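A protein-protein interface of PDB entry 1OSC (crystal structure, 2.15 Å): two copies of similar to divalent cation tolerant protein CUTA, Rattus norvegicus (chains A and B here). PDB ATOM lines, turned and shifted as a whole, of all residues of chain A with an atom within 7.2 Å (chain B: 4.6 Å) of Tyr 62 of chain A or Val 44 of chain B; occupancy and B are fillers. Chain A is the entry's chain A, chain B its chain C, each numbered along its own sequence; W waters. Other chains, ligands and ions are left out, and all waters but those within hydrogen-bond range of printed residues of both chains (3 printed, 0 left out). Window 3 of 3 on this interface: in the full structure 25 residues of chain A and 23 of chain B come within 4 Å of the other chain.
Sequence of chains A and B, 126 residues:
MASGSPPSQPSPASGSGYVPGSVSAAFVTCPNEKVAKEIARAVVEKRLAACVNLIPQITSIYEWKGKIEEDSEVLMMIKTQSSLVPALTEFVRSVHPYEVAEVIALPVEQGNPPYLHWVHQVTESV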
ATOM      1  N   SER A  60      21.512  20.187 -31.543  1.00  0.00           N
ATOM      2  CA  SER A  60      21.029  20.219 -30.194  1.00  0.00           C
ATOM      3  C   SER A  60      21.441  19.007 -29.394  1.00  0.00           C
ATOM      4  O   SER A  60      21.323  17.889 -29.877  1.00  0.00           O
ATOM      5  CB  SER A  60      19.490  20.202 -30.205  1.00  0.00           C
ATOM      6  OG  SER A  60      19.126  21.284 -31.007  1.00  0.00           O
ATOM      7  N   ILE A  61      21.835  19.286 -28.175  1.00  0.00           N
ATOM      8  CA  ILE A  61      22.439  18.438 -27.247  1.00  0.00           C
ATOM      9  C   ILE A  61      21.694  18.573 -25.952  1.00  0.00           C
ATOM     10  O   ILE A  61      21.562  19.719 -25.372  1.00  0.00           O
ATOM     11  CB  ILE A  61      23.970  18.800 -27.059  1.00  0.00           C
ATOM     12  CG1 ILE A  61      24.757  18.423 -28.322  1.00  0.00           C
ATOM     13  CG2 ILE A  61      24.493  17.891 -25.987  1.00  0.00           C
ATOM     14  CD1 ILE A  61      25.928  19.310 -28.736  1.00  0.00           C
ATOM     15  N   TYR A  62      21.213  17.441 -25.449  1.00  0.00           N
ATOM     16  CA  TYR A  62      20.491  17.415 -24.179  1.00  0.00           C
ATOM     17  C   TYR A  62      20.471  15.969 -23.698  1.00  0.00           C
ATOM     18  O   TYR A  62      20.686  15.072 -24.506  1.00  0.00           O
ATOM     19  CB  TYR A  62      19.001  17.816 -24.382  1.00  0.00           C
ATOM     20  CG  TYR A  62      18.307  17.036 -25.432  1.00  0.00           C
ATOM     21  CD1 TYR A  62      18.568  17.269 -26.741  1.00  0.00           C
ATOM     22  CD2 TYR A  62      17.461  15.975 -25.086  1.00  0.00           C
ATOM     23  CE1 TYR A  62      17.984  16.537 -27.740  1.00  0.00           C
ATOM     24  CE2 TYR A  62      16.883  15.209 -26.018  1.00  0.00           C
ATOM     25  CZ  TYR A  62      17.109  15.502 -27.344  1.00  0.00           C
ATOM     26  OH  TYR A  62      16.459  14.748 -28.307  1.00  0.00           O
ATOM     27  N   GLU A  63      20.078  15.778 -22.453  1.00  0.00           N
ATOM     28  CA  GLU A  63      19.754  14.481 -21.848  1.00  0.00           C
ATOM     29  C   GLU A  63      18.437  13.854 -22.203  1.00  0.00           C
ATOM     30  O   GLU A  63      17.378  14.473 -22.152  1.00  0.00           O
ATOM     31  CB  GLU A  63      19.759  14.549 -20.328  1.00  0.00           C
ATOM     32  CG  GLU A  63      21.161  14.778 -19.702  1.00  0.00           C
ATOM     33  CD  GLU A  63      22.077  13.544 -19.661  1.00  0.00           C
ATOM     34  OE1 GLU A  63      21.608  12.439 -19.964  1.00  0.00           O
ATOM     35  OE2 GLU A  63      23.278  13.679 -19.331  1.00  0.00           O
ATOM     36  N   TRP A  64      18.476  12.559 -22.538  1.00  0.00           N
ATOM     37  CA  TRP A  64      17.222  11.863 -22.740  1.00  0.00           C
ATOM     38  C   TRP A  64      17.347  10.550 -22.011  1.00  0.00           C
ATOM     39  O   TRP A  64      18.298   9.768 -22.242  1.00  0.00           O
ATOM     40  CB  TRP A  64      16.970  11.712 -24.231  1.00  0.00           C
ATOM     41  CG  TRP A  64      15.828  10.847 -24.486  1.00  0.00           C
ATOM     42  CD1 TRP A  64      15.848   9.530 -24.906  1.00  0.00           C
ATOM     43  CD2 TRP A  64      14.456  11.188 -24.302  1.00  0.00           C
ATOM     44  NE1 TRP A  64      14.560   9.053 -25.006  1.00  0.00           N
ATOM     45  CE2 TRP A  64      13.690  10.039 -24.618  1.00  0.00           C
ATOM     46  CE3 TRP A  64      13.787  12.365 -23.911  1.00  0.00           C
ATOM     47  CZ2 TRP A  64      12.305  10.038 -24.596  1.00  0.00           C
ATOM     48  CZ3 TRP A  64      12.404  12.353 -23.837  1.00  0.00           C
ATOM     49  CH2 TRP A  64      11.672  11.208 -24.191  1.00  0.00           C
ATOM     50  N   LYS A  65      16.451  10.367 -21.059  1.00  0.00           N
ATOM     51  CA  LYS A  65      16.339   9.134 -20.262  1.00  0.00           C
ATOM     52  C   LYS A  65      17.712   8.799 -19.754  1.00  0.00           C
ATOM     53  O   LYS A  65      18.172   7.639 -19.851  1.00  0.00           O
ATOM     54  CB  LYS A  65      15.785   7.962 -21.102  1.00  0.00           C
ATOM     55  CG  LYS A  65      14.261   8.059 -21.459  1.00  0.00           C
ATOM     56  CD  LYS A  65      13.800   6.751 -22.060  1.00  0.00           C
ATOM     57  CE  LYS A  65      12.279   6.675 -22.248  1.00  0.00           C
ATOM     58  NZ  LYS A  65      11.737   5.261 -22.438  1.00  0.00           N
ATOM     59  N   LYS A  67      20.804  10.053 -20.852  1.00  0.00           N
ATOM     60  CA  LYS A  67      21.919   9.867 -21.771  1.00  0.00           C
ATOM     61  C   LYS A  67      22.059  11.005 -22.812  1.00  0.00           C
ATOM     62  O   LYS A  67      21.122  11.385 -23.411  1.00  0.00           O
ATOM     63  CB  LYS A  67      21.710   8.510 -22.521  1.00  0.00           C
ATOM     64  CG  LYS A  67      21.875   7.201 -21.656  1.00  0.00           C
ATOM     65  CD  LYS A  67      23.373   6.894 -21.274  1.00  0.00           C
ATOM     66  CE  LYS A  67      24.184   6.347 -22.484  1.00  0.00           C
ATOM     67  NZ  LYS A  67      24.815   4.976 -22.308  1.00  0.00           N
ATOM     68  N   ILE A  68      23.258  11.468 -23.111  1.00  0.00           N
ATOM     69  CA  ILE A  68      23.374  12.521 -24.075  1.00  0.00           C
ATOM     70  C   ILE A  68      22.901  12.229 -25.506  1.00  0.00           C
ATOM     71  O   ILE A  68      23.384  11.277 -26.124  1.00  0.00           O
ATOM     72  CB  ILE A  68      24.753  13.046 -24.106  1.00  0.00           C
ATOM     73  CG1 ILE A  68      25.048  13.840 -22.834  1.00  0.00           C
ATOM     74  CG2 ILE A  68      24.910  13.978 -25.324  1.00  0.00           C
ATOM     75  CD1 ILE A  68      26.282  14.742 -23.020  1.00  0.00           C
ATOM     76  N   GLU A  69      21.990  13.049 -26.055  1.00  0.00           N
ATOM     77  CA  GLU A  69      21.666  13.003 -27.518  1.00  0.00           C
ATOM     78  C   GLU A  69      22.207  14.179 -28.297  1.00  0.00           C
ATOM     79  O   GLU A  69      22.450  15.212 -27.687  1.00  0.00           O
ATOM     80  CB  GLU A  69      20.188  13.121 -27.795  1.00  0.00           C
ATOM     81  CG  GLU A  69      19.370  12.058 -27.209  1.00  0.00           C
ATOM     82  CD  GLU A  69      18.757  11.133 -28.250  1.00  0.00           C
ATOM     83  OE1 GLU A  69      18.809  11.309 -29.526  1.00  0.00           O
ATOM     84  OE2 GLU A  69      18.186  10.211 -27.685  1.00  0.00           O
ATOM     85  N   GLU A  70      22.337  14.042 -29.630  1.00  0.00           N
ATOM     86  CA  GLU A  70      22.553  15.160 -30.556  1.00  0.00           C
ATOM     87  C   GLU A  70      21.634  15.057 -31.740  1.00  0.00           C
ATOM     88  O   GLU A  70      21.637  14.050 -32.459  1.00  0.00           O
ATOM     89  CB  GLU A  70      23.968  15.253 -31.029  1.00  0.00           C
ATOM     90  CG  GLU A  70      24.988  14.751 -30.008  1.00  0.00           C
ATOM     91  CD  GLU A  70      26.370  15.157 -30.392  1.00  0.00           C
ATOM     92  OE1 GLU A  70      26.530  15.455 -31.652  1.00  0.00           O
ATOM     93  OE2 GLU A  70      27.266  15.210 -29.427  1.00  0.00           O
ATOM     94  N   ASP A  71      20.823  16.074 -31.953  1.00  0.00           N
ATOM     95  CA  ASP A  71      19.847  16.050 -33.036  1.00  0.00           C
ATOM     96  C   ASP A  71      20.243  17.078 -34.027  1.00  0.00           C
ATOM     97  O   ASP A  71      20.798  18.062 -33.708  1.00  0.00           O
ATOM     98  CB  ASP A  71      18.432  16.353 -32.574  1.00  0.00           C
ATOM     99  CG  ASP A  71      17.853  15.251 -31.738  1.00  0.00           C
ATOM    100  OD1 ASP A  71      18.627  14.350 -31.385  1.00  0.00           O
ATOM    101  OD2 ASP A  71      16.672  15.210 -31.322  1.00  0.00           O
ATOM    102  N   GLU A  73      18.716  19.959 -36.103  1.00  0.00           N
ATOM    103  CA  GLU A  73      17.459  20.725 -36.182  1.00  0.00           C
ATOM    104  C   GLU A  73      17.553  22.085 -36.894  1.00  0.00           C
ATOM    105  O   GLU A  73      18.606  22.444 -37.427  1.00  0.00           O
ATOM    106  CB  GLU A  73      16.993  21.030 -34.813  1.00  0.00           C
ATOM    107  CG  GLU A  73      17.418  20.058 -33.756  1.00  0.00           C
ATOM    108  CD  GLU A  73      16.251  19.718 -32.928  1.00  0.00           C
ATOM    109  OE1 GLU A  73      15.372  19.022 -33.468  1.00  0.00           O
ATOM    110  OE2 GLU A  73      16.181  20.205 -31.781  1.00  0.00           O
ATOM    111  N   TYR A  98       7.628  17.289 -31.831  1.00  0.00           N
ATOM    112  CA  TYR A  98       7.373  16.367 -30.732  1.00  0.00           C
ATOM    113  C   TYR A  98       6.280  16.640 -29.708  1.00  0.00           C
ATOM    114  O   TYR A  98       5.467  17.546 -29.823  1.00  0.00           O
ATOM    115  CB  TYR A  98       8.720  16.231 -29.939  1.00  0.00           C
ATOM    116  CG  TYR A  98       9.064  14.790 -29.576  1.00  0.00           C
ATOM    117  CD1 TYR A  98      10.214  14.167 -30.072  1.00  0.00           C
ATOM    118  CD2 TYR A  98       8.197  14.039 -28.773  1.00  0.00           C
ATOM    119  CE1 TYR A  98      10.493  12.816 -29.746  1.00  0.00           C
ATOM    120  CE2 TYR A  98       8.452  12.708 -28.444  1.00  0.00           C
ATOM    121  CZ  TYR A  98       9.600  12.083 -28.922  1.00  0.00           C
ATOM    122  OH  TYR A  98       9.818  10.740 -28.562  1.00  0.00           O
ATOM    123  N   GLU A 102       9.490  23.065 -27.740  1.00  0.00           N
ATOM    124  CA  GLU A 102      10.359  23.947 -27.058  1.00  0.00           C
ATOM    125  C   GLU A 102      10.032  25.366 -27.613  1.00  0.00           C
ATOM    126  O   GLU A 102      10.332  25.648 -28.754  1.00  0.00           O
ATOM    127  CB  GLU A 102      11.809  23.468 -27.392  1.00  0.00           C
ATOM    128  CG  GLU A 102      12.053  22.074 -26.742  1.00  0.00           C
ATOM    129  CD  GLU A 102      12.650  20.907 -27.607  1.00  0.00           C
ATOM    130  OE1 GLU A 102      12.268  19.728 -27.282  1.00  0.00           O
ATOM    131  OE2 GLU A 102      13.500  21.129 -28.561  1.00  0.00           O
ATOM    132  N   ALA B  40      29.397  21.816 -24.738  1.00  0.00           N
ATOM    133  CA  ALA B  40      27.952  21.592 -24.728  1.00  0.00           C
ATOM    134  C   ALA B  40      27.674  20.304 -23.995  1.00  0.00           C
ATOM    135  O   ALA B  40      26.744  20.230 -23.134  1.00  0.00           O
ATOM    136  CB  ALA B  40      27.378  21.529 -26.145  1.00  0.00           C
ATOM    137  N   ARG B  41      28.466  19.261 -24.319  1.00  0.00           N
ATOM    138  CA  ARG B  41      28.240  17.941 -23.691  1.00  0.00           C
ATOM    139  C   ARG B  41      28.490  17.998 -22.194  1.00  0.00           C
ATOM    140  O   ARG B  41      27.739  17.420 -21.411  1.00  0.00           O
ATOM    141  CB  ARG B  41      29.181  16.900 -24.312  1.00  0.00           C
ATOM    142  CG  ARG B  41      28.679  16.411 -25.666  1.00  0.00           C
ATOM    143  CD  ARG B  41      29.559  15.280 -26.308  1.00  0.00           C
ATOM    144  NE  ARG B  41      28.686  14.481 -27.136  1.00  0.00           N
ATOM    145  CZ  ARG B  41      28.116  13.331 -26.752  1.00  0.00           C
ATOM    146  NH1 ARG B  41      28.399  12.789 -25.565  1.00  0.00           N
ATOM    147  NH2 ARG B  41      27.287  12.706 -27.587  1.00  0.00           N
ATOM    148  N   ALA B  42      29.585  18.629 -21.817  1.00  0.00           N
ATOM    149  CA  ALA B  42      29.893  18.758 -20.412  1.00  0.00           C
ATOM    150  C   ALA B  42      28.835  19.531 -19.617  1.00  0.00           C
ATOM    151  O   ALA B  42      28.562  19.143 -18.487  1.00  0.00           O
ATOM    152  CB  ALA B  42      31.287  19.438 -20.233  1.00  0.00           C
ATOM    153  N   VAL B  43      28.256  20.655 -20.118  1.00  0.00           N
ATOM    154  CA  VAL B  43      27.241  21.360 -19.244  1.00  0.00           C
ATOM    155  C   VAL B  43      25.948  20.612 -19.040  1.00  0.00           C
ATOM    156  O   VAL B  43      25.250  20.702 -17.989  1.00  0.00           O
ATOM    157  CB  VAL B  43      26.930  22.866 -19.619  1.00  0.00           C
ATOM    158  CG1 VAL B  43      28.214  23.722 -19.742  1.00  0.00           C
ATOM    159  CG2 VAL B  43      25.995  23.001 -20.824  1.00  0.00           C
ATOM    160  N   VAL B  44      25.600  19.857 -20.044  1.00  0.00           N
ATOM    161  CA  VAL B  44      24.364  19.063 -20.017  1.00  0.00           C
ATOM    162  C   VAL B  44      24.527  17.911 -19.015  1.00  0.00           C
ATOM    163  O   VAL B  44      23.684  17.750 -18.090  1.00  0.00           O
ATOM    164  CB  VAL B  44      24.148  18.642 -21.420  1.00  0.00           C
ATOM    165  CG1 VAL B  44      23.248  17.440 -21.554  1.00  0.00           C
ATOM    166  CG2 VAL B  44      23.539  19.887 -22.145  1.00  0.00           C
ATOM    167  N   GLU B  45      25.658  17.189 -19.172  1.00  0.00           N
ATOM    168  CA  GLU B  45      26.122  16.113 -18.253  1.00  0.00           C
ATOM    169  C   GLU B  45      26.221  16.510 -16.817  1.00  0.00           C
ATOM    170  O   GLU B  45      25.713  15.812 -15.927  1.00  0.00           O
ATOM    171  CB  GLU B  45      27.522  15.586 -18.680  1.00  0.00           C
ATOM    172  CG  GLU B  45      27.441  14.166 -19.245  1.00  0.00           C
ATOM    173  CD  GLU B  45      28.811  13.567 -19.751  1.00  0.00           C
ATOM    174  OE1 GLU B  45      29.859  14.311 -19.939  1.00  0.00           O
ATOM    175  OE2 GLU B  45      28.814  12.330 -20.002  1.00  0.00           O
ATOM    176  N   LYS B  46      26.910  17.609 -16.565  1.00  0.00           N
ATOM    177  CA  LYS B  46      26.830  18.214 -15.204  1.00  0.00           C
ATOM    178  C   LYS B  46      25.448  18.833 -14.795  1.00  0.00           C
ATOM    179  O   LYS B  46      25.297  19.305 -13.661  1.00  0.00           O
ATOM    180  CB  LYS B  46      27.951  19.228 -14.978  1.00  0.00           C
ATOM    181  CG  LYS B  46      29.264  18.824 -15.563  1.00  0.00           C
ATOM    182  CD  LYS B  46      30.295  19.892 -15.254  1.00  0.00           C
ATOM    183  CE  LYS B  46      31.403  19.303 -14.283  1.00  0.00           C
ATOM    184  NZ  LYS B  46      32.274  18.390 -15.162  1.00  0.00           N
ATOM    185  N   ARG B  47      24.425  18.730 -15.643  1.00  0.00           N
ATOM    186  CA  ARG B  47      23.115  19.415 -15.293  1.00  0.00           C
ATOM    187  C   ARG B  47      23.247  20.930 -14.924  1.00  0.00           C
ATOM    188  O   ARG B  47      22.529  21.433 -14.093  1.00  0.00           O
ATOM    189  CB  ARG B  47      22.331  18.662 -14.187  1.00  0.00           C
ATOM    190  CG  ARG B  47      22.310  17.118 -14.382  1.00  0.00           C
ATOM    191  CD  ARG B  47      21.349  16.279 -13.443  1.00  0.00           C
ATOM    192  NE  ARG B  47      20.734  16.985 -12.323  1.00  0.00           N
ATOM    193  CZ  ARG B  47      19.429  16.965 -11.999  1.00  0.00           C
ATOM    194  NH1 ARG B  47      18.996  17.634 -10.909  1.00  0.00           N
ATOM    195  NH2 ARG B  47      18.556  16.316 -12.760  1.00  0.00           N
ATOM    196  N   ALA B  49      22.792  22.852 -17.494  1.00  0.00           N
ATOM    197  CA  ALA B  49      21.982  23.263 -18.593  1.00  0.00           C
ATOM    198  C   ALA B  49      21.079  22.136 -18.949  1.00  0.00           C
ATOM    199  O   ALA B  49      21.416  20.944 -18.726  1.00  0.00           O
ATOM    200  CB  ALA B  49      22.790  23.594 -19.731  1.00  0.00           C
ATOM    201  N   ALA B  50      19.921  22.489 -19.521  1.00  0.00           N
ATOM    202  CA  ALA B  50      19.034  21.477 -19.983  1.00  0.00           C
ATOM    203  C   ALA B  50      19.244  21.174 -21.446  1.00  0.00           C
ATOM    204  O   ALA B  50      18.992  20.038 -21.905  1.00  0.00           O
ATOM    205  CB  ALA B  50      17.571  21.926 -19.748  1.00  0.00           C
ATOM    206  N   CYS B  51      19.640  22.178 -22.235  1.00  0.00           N
ATOM    207  CA  CYS B  51      19.578  21.992 -23.687  1.00  0.00           C
ATOM    208  C   CYS B  51      20.545  22.993 -24.209  1.00  0.00           C
ATOM    209  O   CYS B  51      20.643  24.104 -23.638  1.00  0.00           O
ATOM    210  CB  CYS B  51      18.159  22.283 -24.250  1.00  0.00           C
ATOM    211  SG  CYS B  51      18.244  21.957 -26.007  1.00  0.00           S
ATOM    212  N   VAL B  52      21.272  22.630 -25.261  1.00  0.00           N
ATOM    213  CA  VAL B  52      22.190  23.522 -25.922  1.00  0.00           C
ATOM    214  C   VAL B  52      21.985  23.471 -27.447  1.00  0.00           C
ATOM    215  O   VAL B  52      21.873  22.360 -28.004  1.00  0.00           O
ATOM    216  CB  VAL B  52      23.652  23.108 -25.696  1.00  0.00           C
ATOM    217  CG1 VAL B  52      24.570  24.223 -26.427  1.00  0.00           C
ATOM    218  CG2 VAL B  52      23.975  23.019 -24.180  1.00  0.00           C
ATOM    219  N   TRP B 118      10.306  21.025 -17.699  1.00  0.00           N
ATOM    220  CA  TRP B 118      11.324  20.083 -18.078  1.00  0.00           C
ATOM    221  C   TRP B 118      12.717  20.715 -17.902  1.00  0.00           C
ATOM    222  O   TRP B 118      13.610  20.075 -17.304  1.00  0.00           O
ATOM    223  CB  TRP B 118      11.113  19.585 -19.511  1.00  0.00           C
ATOM    224  CG  TRP B 118      12.250  18.732 -19.943  1.00  0.00           C
ATOM    225  CD1 TRP B 118      12.444  17.395 -19.606  1.00  0.00           C
ATOM    226  CD2 TRP B 118      13.424  19.125 -20.687  1.00  0.00           C
ATOM    227  NE1 TRP B 118      13.613  16.938 -20.174  1.00  0.00           N
ATOM    228  CE2 TRP B 118      14.243  17.957 -20.825  1.00  0.00           C
ATOM    229  CE3 TRP B 118      13.846  20.323 -21.311  1.00  0.00           C
ATOM    230  CZ2 TRP B 118      15.435  17.959 -21.506  1.00  0.00           C
ATOM    231  CZ3 TRP B 118      15.053  20.318 -22.037  1.00  0.00           C
ATOM    232  CH2 TRP B 118      15.835  19.168 -22.103  1.00  0.00           C
HETATM  233  O   HOH W   1      15.445  19.665 -26.149  1.00  0.00           O
HETATM  234  O   HOH W   2      19.276  17.614 -20.433  1.00  0.00           O
HETATM  235  O   HOH W   3      16.020  22.727 -27.975  1.00  0.00           O
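The backbone carbonyl oxygen of Ile 61 of chain A sits at hydrogen-bond distance from the backbone NH of Val 52 of chain B. The side-chain carboxylate (OE2) of Glu 70 of chain A lies within salt-bridge range of the guanidinium group (NE) of Arg 41 of chain B (2.8 Å).
The backbone NH of Asp 71 of chain A lies within hydrogen-bond range of the backbone carbonyl oxygen of Ser 60 of chain A (2.8 Å). The side-chain hydroxyl (OG) of Ser 60 of chain A sits at hydrogen-bond distance from the side-chain carboxylate (OE2) of Glu 73 of chain A, at 3.2 Å. The backbone carbonyl oxygen (O) of Tyr 62 of chain A lies within hydrogen-bond range of the backbone NH (N) of Glu 69 of chain A, 2.9 Å away. The side-chain hydroxyl (OH) of Tyr 62 of chain A lies within hydrogen-bond range of the side-chain carboxylate (OD2) of Asp 71 of chain A (3.1 Å). The side-chain carboxylate (OE1) of Glu 63 of chain A is in hydrogen-bond range of the backbone NH (N) of Lys 67 of chain A, at 2.7 Å.
Among the printed residues, pairs that only touch across the chains: Ser 60 of chain A with Val 52 of chain B (3.2 Å), Ile 61 of chain A with Ala 40 of chain B (3.7 Å), Ile 61 of chain A with Val 44 of chain B (3.8 Å), Ile 61 of chain A with Cys 51 of chain B (3.5 Å), Tyr 62 of chain A with Val 44 of chain B (3.8 Å), Tyr 62 of chain A with Ala 50 of chain B (3.3 Å), Glu 63 of chain A with Val 44 of chain B (3.7 Å), Glu 63 of chain A with Glu 45 of chain B (3.9 Å), Ile 68 of chain A with Arg 41 of chain B (3.4 Å) and Ile 68 of chain A with Glu 45 of chain B (3.99 Å).
Tyr 62 of chain A touches two residues of chain B. Val 44 of chain B touches just these residues of chain A: Ile 61 (3.8 Å), Tyr 62 (3.8 Å) and Glu 63 (3.7 Å). Printed residues of chain B within 4 Å of Ser 60 of chain A: Val 52 (3.2 Å). Printed residues of chain A within 4 Å of Ala 50 of chain B: Tyr 62. Glu 73 of chain A touches none of the printed residues of chain B. Tyr 98 of chain A touches none of the printed residues of chain B.
Printed residues of chain A that touch a printed residue of chain B: Ser 60, Ile 61, Tyr 62, Glu 63, Ile 68 and Glu 70.
No position is printed for both chains. Of the 12 pairs that touch across the chains among the printed residues, none has its exchanged pair printed and touching as well.
Water W2 bridges N of Glu 63 of chain A (2.8 Å) and O of Ala 50 of chain B (2.9 Å). Water W3 bridges OE2 of Glu 102 of chain A and SG of Cys 51 of chain B. Water W1 bridges the side-chain carboxylate (OE1) of Glu 102 of chain A (3.4 Å) and the side-chain sulfur (SG) of Cys 51 of chain B (3.6 Å).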
